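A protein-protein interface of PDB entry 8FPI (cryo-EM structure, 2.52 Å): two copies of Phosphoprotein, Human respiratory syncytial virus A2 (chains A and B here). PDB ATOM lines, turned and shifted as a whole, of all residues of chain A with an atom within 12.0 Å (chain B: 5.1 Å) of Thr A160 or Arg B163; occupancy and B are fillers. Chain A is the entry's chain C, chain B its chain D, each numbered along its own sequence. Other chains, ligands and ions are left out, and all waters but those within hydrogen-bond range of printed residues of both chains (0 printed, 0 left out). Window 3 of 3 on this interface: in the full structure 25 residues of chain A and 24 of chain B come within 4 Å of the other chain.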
ATOM      1  N   LEU A 152      -9.253  -9.130  -5.582  1.00  0.00           N
ATOM      2  CA  LEU A 152     -10.674  -9.362  -5.415  1.00  0.00           C
ATOM      3  C   LEU A 152     -11.455  -9.166  -6.704  1.00  0.00           C
ATOM      4  O   LEU A 152     -12.476  -9.833  -6.893  1.00  0.00           O
ATOM      5  CB  LEU A 152     -11.232  -8.447  -4.326  1.00  0.00           C
ATOM      6  CG  LEU A 152     -12.729  -8.532  -4.071  1.00  0.00           C
ATOM      7  CD1 LEU A 152     -13.048  -9.866  -3.477  1.00  0.00           C
ATOM      8  CD2 LEU A 152     -13.146  -7.450  -3.134  1.00  0.00           C
ATOM      9  N   VAL A 153     -11.025  -8.259  -7.584  1.00  0.00           N
ATOM     10  CA  VAL A 153     -11.685  -8.126  -8.881  1.00  0.00           C
ATOM     11  C   VAL A 153     -11.368  -9.323  -9.762  1.00  0.00           C
ATOM     12  O   VAL A 153     -12.246  -9.861 -10.437  1.00  0.00           O
ATOM     13  CB  VAL A 153     -11.280  -6.808  -9.563  1.00  0.00           C
ATOM     14  CG1 VAL A 153     -11.806  -6.771 -10.981  1.00  0.00           C
ATOM     15  CG2 VAL A 153     -11.804  -5.626  -8.796  1.00  0.00           C
ATOM     16  N   VAL A 154     -10.113  -9.756  -9.768  1.00  0.00           N
ATOM     17  CA  VAL A 154      -9.710 -10.871 -10.614  1.00  0.00           C
ATOM     18  C   VAL A 154     -10.483 -12.125 -10.229  1.00  0.00           C
ATOM     19  O   VAL A 154     -11.006 -12.842 -11.087  1.00  0.00           O
ATOM     20  CB  VAL A 154      -8.189 -11.084 -10.519  1.00  0.00           C
ATOM     21  CG1 VAL A 154      -7.754 -12.300 -11.296  1.00  0.00           C
ATOM     22  CG2 VAL A 154      -7.474  -9.869 -11.026  1.00  0.00           C
ATOM     23  N   ALA A 155     -10.576 -12.401  -8.926  1.00  0.00           N
ATOM     24  CA  ALA A 155     -11.281 -13.583  -8.445  1.00  0.00           C
ATOM     25  C   ALA A 155     -12.791 -13.454  -8.543  1.00  0.00           C
ATOM     26  O   ALA A 155     -13.475 -14.471  -8.669  1.00  0.00           O
ATOM     27  CB  ALA A 155     -10.892 -13.870  -6.998  1.00  0.00           C
ATOM     28  N   SER A 156     -13.328 -12.243  -8.498  1.00  0.00           N
ATOM     29  CA  SER A 156     -14.764 -12.030  -8.544  1.00  0.00           C
ATOM     30  C   SER A 156     -15.300 -11.984  -9.969  1.00  0.00           C
ATOM     31  O   SER A 156     -16.511 -11.862 -10.159  1.00  0.00           O
ATOM     32  CB  SER A 156     -15.119 -10.742  -7.804  1.00  0.00           C
ATOM     33  OG  SER A 156     -16.449 -10.364  -8.081  1.00  0.00           O
ATOM     34  N   ALA A 157     -14.432 -12.078 -10.970  1.00  0.00           N
ATOM     35  CA  ALA A 157     -14.832 -12.141 -12.373  1.00  0.00           C
ATOM     36  C   ALA A 157     -14.537 -13.554 -12.843  1.00  0.00           C
ATOM     37  O   ALA A 157     -13.472 -13.809 -13.407  1.00  0.00           O
ATOM     38  CB  ALA A 157     -14.082 -11.121 -13.222  1.00  0.00           C
ATOM     39  N   GLY A 158     -15.477 -14.465 -12.627  1.00  0.00           N
ATOM     40  CA  GLY A 158     -15.215 -15.867 -12.818  1.00  0.00           C
ATOM     41  C   GLY A 158     -16.293 -16.574 -13.601  1.00  0.00           C
ATOM     42  O   GLY A 158     -16.890 -16.004 -14.515  1.00  0.00           O
ATOM     43  N   PRO A 159     -16.579 -17.829 -13.245  1.00  0.00           N
ATOM     44  CA  PRO A 159     -17.442 -18.650 -14.105  1.00  0.00           C
ATOM     45  C   PRO A 159     -18.760 -17.997 -14.425  1.00  0.00           C
ATOM     46  O   PRO A 159     -19.305 -18.218 -15.508  1.00  0.00           O
ATOM     47  CB  PRO A 159     -17.633 -19.923 -13.280  1.00  0.00           C
ATOM     48  CG  PRO A 159     -16.481 -19.969 -12.379  1.00  0.00           C
ATOM     49  CD  PRO A 159     -16.144 -18.570 -12.052  1.00  0.00           C
ATOM     50  N   THR A 160     -19.294 -17.193 -13.516  1.00  0.00           N
ATOM     51  CA  THR A 160     -20.593 -16.575 -13.715  1.00  0.00           C
ATOM     52  C   THR A 160     -20.515 -15.227 -14.416  1.00  0.00           C
ATOM     53  O   THR A 160     -21.541 -14.734 -14.889  1.00  0.00           O
ATOM     54  CB  THR A 160     -21.316 -16.425 -12.373  1.00  0.00           C
ATOM     55  OG1 THR A 160     -22.456 -15.577 -12.537  1.00  0.00           O
ATOM     56  CG2 THR A 160     -20.399 -15.842 -11.325  1.00  0.00           C
ATOM     57  N   SER A 161     -19.331 -14.624 -14.498  1.00  0.00           N
ATOM     58  CA  SER A 161     -19.100 -13.463 -15.345  1.00  0.00           C
ATOM     59  C   SER A 161     -18.843 -13.852 -16.789  1.00  0.00           C
ATOM     60  O   SER A 161     -19.413 -13.250 -17.701  1.00  0.00           O
ATOM     61  CB  SER A 161     -17.914 -12.654 -14.824  1.00  0.00           C
ATOM     62  OG  SER A 161     -17.019 -13.485 -14.116  1.00  0.00           O
ATOM     63  N   ALA A 162     -18.003 -14.858 -17.017  1.00  0.00           N
ATOM     64  CA  ALA A 162     -17.862 -15.398 -18.360  1.00  0.00           C
ATOM     65  C   ALA A 162     -19.216 -15.815 -18.918  1.00  0.00           C
ATOM     66  O   ALA A 162     -19.502 -15.606 -20.101  1.00  0.00           O
ATOM     67  CB  ALA A 162     -16.892 -16.574 -18.345  1.00  0.00           C
ATOM     68  N   ARG A 163     -20.071 -16.401 -18.077  1.00  0.00           N
ATOM     69  CA  ARG A 163     -21.397 -16.800 -18.532  1.00  0.00           C
ATOM     70  C   ARG A 163     -22.223 -15.598 -18.962  1.00  0.00           C
ATOM     71  O   ARG A 163     -22.928 -15.655 -19.974  1.00  0.00           O
ATOM     72  CB  ARG A 163     -22.122 -17.571 -17.434  1.00  0.00           C
ATOM     73  CG  ARG A 163     -23.495 -18.093 -17.830  1.00  0.00           C
ATOM     74  CD  ARG A 163     -24.569 -17.619 -16.870  1.00  0.00           C
ATOM     75  NE  ARG A 163     -24.266 -18.013 -15.498  1.00  0.00           N
ATOM     76  CZ  ARG A 163     -24.613 -17.329 -14.414  1.00  0.00           C
ATOM     77  NH1 ARG A 163     -25.288 -16.196 -14.515  1.00  0.00           N
ATOM     78  NH2 ARG A 163     -24.281 -17.786 -13.217  1.00  0.00           N
ATOM     79  N   ASP A 164     -22.160 -14.505 -18.208  1.00  0.00           N
ATOM     80  CA  ASP A 164     -23.009 -13.353 -18.475  1.00  0.00           C
ATOM     81  C   ASP A 164     -22.349 -12.321 -19.377  1.00  0.00           C
ATOM     82  O   ASP A 164     -22.923 -11.248 -19.583  1.00  0.00           O
ATOM     83  CB  ASP A 164     -23.430 -12.694 -17.158  1.00  0.00           C
ATOM     84  CG  ASP A 164     -24.766 -13.212 -16.646  1.00  0.00           C
ATOM     85  OD1 ASP A 164     -25.267 -14.229 -17.169  1.00  0.00           O
ATOM     86  OD2 ASP A 164     -25.320 -12.601 -15.712  1.00  0.00           O
ATOM     87  N   GLY A 165     -21.173 -12.619 -19.922  1.00  0.00           N
ATOM     88  CA  GLY A 165     -20.501 -11.719 -20.836  1.00  0.00           C
ATOM     89  C   GLY A 165     -20.049 -10.447 -20.162  1.00  0.00           C
ATOM     90  O   GLY A 165     -20.179  -9.353 -20.714  1.00  0.00           O
ATOM     91  N   ILE A 166     -19.506 -10.594 -18.955  1.00  0.00           N
ATOM     92  CA  ILE A 166     -19.098  -9.466 -18.133  1.00  0.00           C
ATOM     93  C   ILE A 166     -17.625  -9.508 -17.774  1.00  0.00           C
ATOM     94  O   ILE A 166     -17.090  -8.510 -17.301  1.00  0.00           O
ATOM     95  CB  ILE A 166     -19.973  -9.391 -16.860  1.00  0.00           C
ATOM     96  CG1 ILE A 166     -20.991  -8.271 -16.990  1.00  0.00           C
ATOM     97  CG2 ILE A 166     -19.171  -9.230 -15.585  1.00  0.00           C
ATOM     98  CD1 ILE A 166     -21.811  -8.364 -18.224  1.00  0.00           C
ATOM     99  N   ARG A 167     -16.941 -10.618 -18.017  1.00  0.00           N
ATOM    100  CA  ARG A 167     -15.575 -10.751 -17.537  1.00  0.00           C
ATOM    101  C   ARG A 167     -14.644  -9.751 -18.205  1.00  0.00           C
ATOM    102  O   ARG A 167     -13.720  -9.241 -17.569  1.00  0.00           O
ATOM    103  CB  ARG A 167     -15.077 -12.173 -17.761  1.00  0.00           C
ATOM    104  CG  ARG A 167     -13.997 -12.559 -16.813  1.00  0.00           C
ATOM    105  CD  ARG A 167     -13.633 -13.984 -16.961  1.00  0.00           C
ATOM    106  NE  ARG A 167     -12.366 -14.279 -16.313  1.00  0.00           N
ATOM    107  CZ  ARG A 167     -11.180 -14.025 -16.846  1.00  0.00           C
ATOM    108  NH1 ARG A 167     -11.092 -13.456 -18.031  1.00  0.00           N
ATOM    109  NH2 ARG A 167     -10.077 -14.339 -16.194  1.00  0.00           N
ATOM    110  N   ASP A 168     -14.851  -9.473 -19.490  1.00  0.00           N
ATOM    111  CA  ASP A 168     -13.952  -8.566 -20.193  1.00  0.00           C
ATOM    112  C   ASP A 168     -14.103  -7.135 -19.711  1.00  0.00           C
ATOM    113  O   ASP A 168     -13.116  -6.394 -19.686  1.00  0.00           O
ATOM    114  CB  ASP A 168     -14.200  -8.645 -21.698  1.00  0.00           C
ATOM    115  CG  ASP A 168     -13.468  -9.809 -22.349  1.00  0.00           C
ATOM    116  OD1 ASP A 168     -12.540 -10.368 -21.727  1.00  0.00           O
ATOM    117  OD2 ASP A 168     -13.825 -10.162 -23.492  1.00  0.00           O
ATOM    118  N   ALA A 169     -15.311  -6.730 -19.330  1.00  0.00           N
ATOM    119  CA  ALA A 169     -15.496  -5.423 -18.717  1.00  0.00           C
ATOM    120  C   ALA A 169     -14.863  -5.346 -17.339  1.00  0.00           C
ATOM    121  O   ALA A 169     -14.657  -4.245 -16.825  1.00  0.00           O
ATOM    122  CB  ALA A 169     -16.984  -5.093 -18.616  1.00  0.00           C
ATOM    123  N   MET A 170     -14.543  -6.487 -16.726  1.00  0.00           N
ATOM    124  CA  MET A 170     -13.978  -6.460 -15.384  1.00  0.00           C
ATOM    125  C   MET A 170     -12.466  -6.592 -15.411  1.00  0.00           C
ATOM    126  O   MET A 170     -11.781  -6.010 -14.567  1.00  0.00           O
ATOM    127  CB  MET A 170     -14.584  -7.565 -14.527  1.00  0.00           C
ATOM    128  CG  MET A 170     -16.075  -7.405 -14.272  1.00  0.00           C
ATOM    129  SD  MET A 170     -16.801  -8.846 -13.496  1.00  0.00           S
ATOM    130  CE  MET A 170     -16.025  -8.776 -11.886  1.00  0.00           C
ATOM    131  N   ILE A 171     -11.924  -7.348 -16.362  1.00  0.00           N
ATOM    132  CA  ILE A 171     -10.474  -7.471 -16.470  1.00  0.00           C
ATOM    133  C   ILE A 171      -9.888  -6.600 -17.577  1.00  0.00           C
ATOM    134  O   ILE A 171      -8.660  -6.475 -17.664  1.00  0.00           O
ATOM    135  CB  ILE A 171     -10.036  -8.925 -16.704  1.00  0.00           C
ATOM    136  CG1 ILE A 171     -10.934  -9.605 -17.727  1.00  0.00           C
ATOM    137  CG2 ILE A 171     -10.059  -9.695 -15.400  1.00  0.00           C
ATOM    138  CD1 ILE A 171     -10.215 -10.616 -18.568  1.00  0.00           C
ATOM    139  N   ALA B 155     -20.675  -5.161 -10.646  1.00  0.00           N
ATOM    140  CA  ALA B 155     -20.829  -6.567 -10.991  1.00  0.00           C
ATOM    141  C   ALA B 155     -21.754  -7.254  -9.996  1.00  0.00           C
ATOM    142  O   ALA B 155     -22.716  -7.920 -10.390  1.00  0.00           O
ATOM    143  CB  ALA B 155     -19.469  -7.263 -11.023  1.00  0.00           C
ATOM    144  N   PRO B 159     -28.782  -8.855 -10.730  1.00  0.00           N
ATOM    145  CA  PRO B 159     -28.272  -8.942 -12.103  1.00  0.00           C
ATOM    146  C   PRO B 159     -29.374  -8.868 -13.164  1.00  0.00           C
ATOM    147  O   PRO B 159     -30.529  -8.592 -12.840  1.00  0.00           O
ATOM    148  CB  PRO B 159     -27.593 -10.313 -12.125  1.00  0.00           C
ATOM    149  CG  PRO B 159     -28.314 -11.124 -11.063  1.00  0.00           C
ATOM    150  CD  PRO B 159     -29.175 -10.186 -10.245  1.00  0.00           C
ATOM    151  N   THR B 160     -28.992  -9.100 -14.422  1.00  0.00           N
ATOM    152  CA  THR B 160     -29.914  -9.207 -15.551  1.00  0.00           C
ATOM    153  C   THR B 160     -30.435  -7.845 -15.993  1.00  0.00           C
ATOM    154  O   THR B 160     -31.054  -7.728 -17.056  1.00  0.00           O
ATOM    155  CB  THR B 160     -31.093 -10.119 -15.195  1.00  0.00           C
ATOM    156  OG1 THR B 160     -30.603 -11.352 -14.654  1.00  0.00           O
ATOM    157  CG2 THR B 160     -31.939 -10.414 -16.428  1.00  0.00           C
ATOM    158  N   SER B 161     -30.171  -6.809 -15.203  1.00  0.00           N
ATOM    159  CA  SER B 161     -30.412  -5.434 -15.611  1.00  0.00           C
ATOM    160  C   SER B 161     -29.253  -4.524 -15.240  1.00  0.00           C
ATOM    161  O   SER B 161     -29.141  -3.422 -15.790  1.00  0.00           O
ATOM    162  CB  SER B 161     -31.711  -4.913 -14.988  1.00  0.00           C
ATOM    163  OG  SER B 161     -32.727  -5.901 -15.035  1.00  0.00           O
ATOM    164  N   ALA B 162     -28.389  -4.959 -14.327  1.00  0.00           N
ATOM    165  CA  ALA B 162     -27.112  -4.313 -14.085  1.00  0.00           C
ATOM    166  C   ALA B 162     -25.965  -5.026 -14.779  1.00  0.00           C
ATOM    167  O   ALA B 162     -24.845  -4.509 -14.777  1.00  0.00           O
ATOM    168  CB  ALA B 162     -26.828  -4.237 -12.581  1.00  0.00           C
ATOM    169  N   ARG B 163     -26.216  -6.207 -15.352  1.00  0.00           N
ATOM    170  CA  ARG B 163     -25.235  -6.903 -16.168  1.00  0.00           C
ATOM    171  C   ARG B 163     -25.565  -6.869 -17.652  1.00  0.00           C
ATOM    172  O   ARG B 163     -24.645  -6.785 -18.468  1.00  0.00           O
ATOM    173  CB  ARG B 163     -25.100  -8.364 -15.715  1.00  0.00           C
ATOM    174  CG  ARG B 163     -24.259  -8.526 -14.458  1.00  0.00           C
ATOM    175  CD  ARG B 163     -24.098  -9.976 -14.051  1.00  0.00           C
ATOM    176  NE  ARG B 163     -23.021 -10.146 -13.081  1.00  0.00           N
ATOM    177  CZ  ARG B 163     -22.592 -11.320 -12.631  1.00  0.00           C
ATOM    178  NH1 ARG B 163     -21.605 -11.375 -11.751  1.00  0.00           N
ATOM    179  NH2 ARG B 163     -23.150 -12.441 -13.057  1.00  0.00           N
ATOM    180  N   ASP B 164     -26.844  -6.908 -18.023  1.00  0.00           N
ATOM    181  CA  ASP B 164     -27.198  -6.657 -19.415  1.00  0.00           C
ATOM    182  C   ASP B 164     -26.662  -5.306 -19.866  1.00  0.00           C
ATOM    183  O   ASP B 164     -26.311  -5.130 -21.038  1.00  0.00           O
ATOM    184  CB  ASP B 164     -28.714  -6.719 -19.595  1.00  0.00           C
ATOM    185  CG  ASP B 164     -29.127  -6.798 -21.053  1.00  0.00           C
ATOM    186  OD1 ASP B 164     -28.635  -5.983 -21.860  1.00  0.00           O
ATOM    187  OD2 ASP B 164     -29.950  -7.673 -21.393  1.00  0.00           O
ATOM    188  N   GLY B 165     -26.591  -4.344 -18.950  1.00  0.00           N
ATOM    189  CA  GLY B 165     -26.037  -3.038 -19.240  1.00  0.00           C
ATOM    190  C   GLY B 165     -24.527  -2.959 -19.202  1.00  0.00           C
ATOM    191  O   GLY B 165     -23.967  -1.947 -19.630  1.00  0.00           O
ATOM    192  N   ILE B 166     -23.852  -3.984 -18.696  1.00  0.00           N
ATOM    193  CA  ILE B 166     -22.406  -4.087 -18.799  1.00  0.00           C
ATOM    194  C   ILE B 166     -22.005  -4.776 -20.101  1.00  0.00           C
ATOM    195  O   ILE B 166     -20.828  -4.835 -20.434  1.00  0.00           O
ATOM    196  CB  ILE B 166     -21.805  -4.809 -17.582  1.00  0.00           C
ATOM    197  CG1 ILE B 166     -22.272  -4.156 -16.284  1.00  0.00           C
ATOM    198  CG2 ILE B 166     -20.288  -4.790 -17.656  1.00  0.00           C
ATOM    199  CD1 ILE B 166     -21.931  -4.958 -15.050  1.00  0.00           C
ATOM    200  N   ARG B 167     -22.978  -5.298 -20.842  1.00  0.00           N
ATOM    201  CA  ARG B 167     -22.741  -5.906 -22.143  1.00  0.00           C
ATOM    202  C   ARG B 167     -23.126  -4.981 -23.283  1.00  0.00           C
ATOM    203  O   ARG B 167     -22.352  -4.821 -24.233  1.00  0.00           O
ATOM    204  CB  ARG B 167     -23.521  -7.226 -22.248  1.00  0.00           C
ATOM    205  CG  ARG B 167     -22.654  -8.463 -22.167  1.00  0.00           C
ATOM    206  CD  ARG B 167     -23.379  -9.676 -22.717  1.00  0.00           C
ATOM    207  NE  ARG B 167     -24.699  -9.843 -22.110  1.00  0.00           N
ATOM    208  CZ  ARG B 167     -25.858  -9.564 -22.701  1.00  0.00           C
ATOM    209  NH1 ARG B 167     -25.898  -9.081 -23.936  1.00  0.00           N
ATOM    210  NH2 ARG B 167     -26.991  -9.764 -22.043  1.00  0.00           N
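NH2 of Arg B163 lies within hydrogen-bond range of OG1 of Thr A160 (3.3 Å).
O of Asp A164 sits at hydrogen-bond distance from NE of Arg B167, at 3.4 Å.
The guanidinium group (NH2) of Arg B163 is in salt-bridge range of the side-chain carboxylate (OD2) of Asp A164 (3.4 Å).
NH2 of Arg A163 is in hydrogen-bond range of OG1 of Thr A160 (2.9 Å).
OD1 of Asp A164 lies within salt-bridge range of NH1 of Arg A163.
The backbone carbonyl oxygen of Ser A161 sits at hydrogen-bond distance from the backbone NH of Ile A166 (2.9 Å).
OD2 of Asp B164 is in salt-bridge range of NH2 of Arg B167.
Among the printed residues, pairs that only touch across the chains: Gly A165 with Arg B167 (3.0 Å), Ile A166 with Arg B163 (3.3 Å), Ala A169 with Ile B166 (3.5 Å), Ile A166 with Ile B166 (3.6 Å) and Met A170 with Ala B155 (3.9 Å).
Arg B163 touches just these residues of chain A: Thr A160, Asp A164 and Ile A166.
No residue of chain A comes within 4 Å of Pro B159.
No residue of chain A comes within 4 Å of Thr B160.
No residue of chain A comes within 4 Å of Ser B161.
No residue of chain A comes within 4 Å of Asp B164.
No residue of chain A comes within 4 Å of Gly B165.
Ile B166 touches two residues of chain A.
Arg B167 touches two residues of chain A.
Printed residues of chain B within 4 Å of Ile A166: Arg B163 and Ile B166.
Of the printed residues of chain B, Met A170 touches Ala B155.
Of the printed residues of chain B, Asp A164 touches Arg B163 (3.3 Å) and Arg B167 (3.4 Å).
Of the printed residues of chain B, Ala A169 touches Ile B166.
Of the printed residues of chain B, Gly A165 touches Arg B167 (3.0 Å).
Leu A152 touches none of the printed residues of chain B.
The nearest printed residue of chain B that does not touch Thr A160 is Pro B159 (7.4 Å).
The nearest printed residue of chain B that does not touch Gly A165 is Ile B166 (4.6 Å).
Printed residues of chain A that touch a printed residue of chain B: Thr A160, Asp A164, Gly A165, Ile A166, Ala A169 and Met A170.
Hydrophobic or aromatic side chains of chain A that line the printed part of chain B: Ile A166, Ala A169 and Met A170.
Along chain A the printed residues that touch a printed residue of chain B span positions 160 to 170.
Hydrophobic or aromatic side chains of chain B that line the printed part of chain A: Ala B155 and Ile B166.
Among the printed residues, 8 pairs touch across the chains.
Asp A164 touches Arg B163, but with the chains exchanged Arg A163 does not touch Asp B164 (9.8 Å).
Asp A164 touches Arg B167, but with the chains exchanged Arg A167 does not touch Asp B164 (10.6 Å).
Gly A165 touches Arg B167, but with the chains exchanged Arg A167 does not touch Gly B165 (10.8 Å).
Ile A166 touches its own counterpart, Ile B166.
Positions printed for both chains: 155, 159, 160, 161, 162, 163, 164, 165, 166 and 167.
Of the 8 pairs that touch across the chains among the printed residues, 1 has its exchanged pair printed and touching as well.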
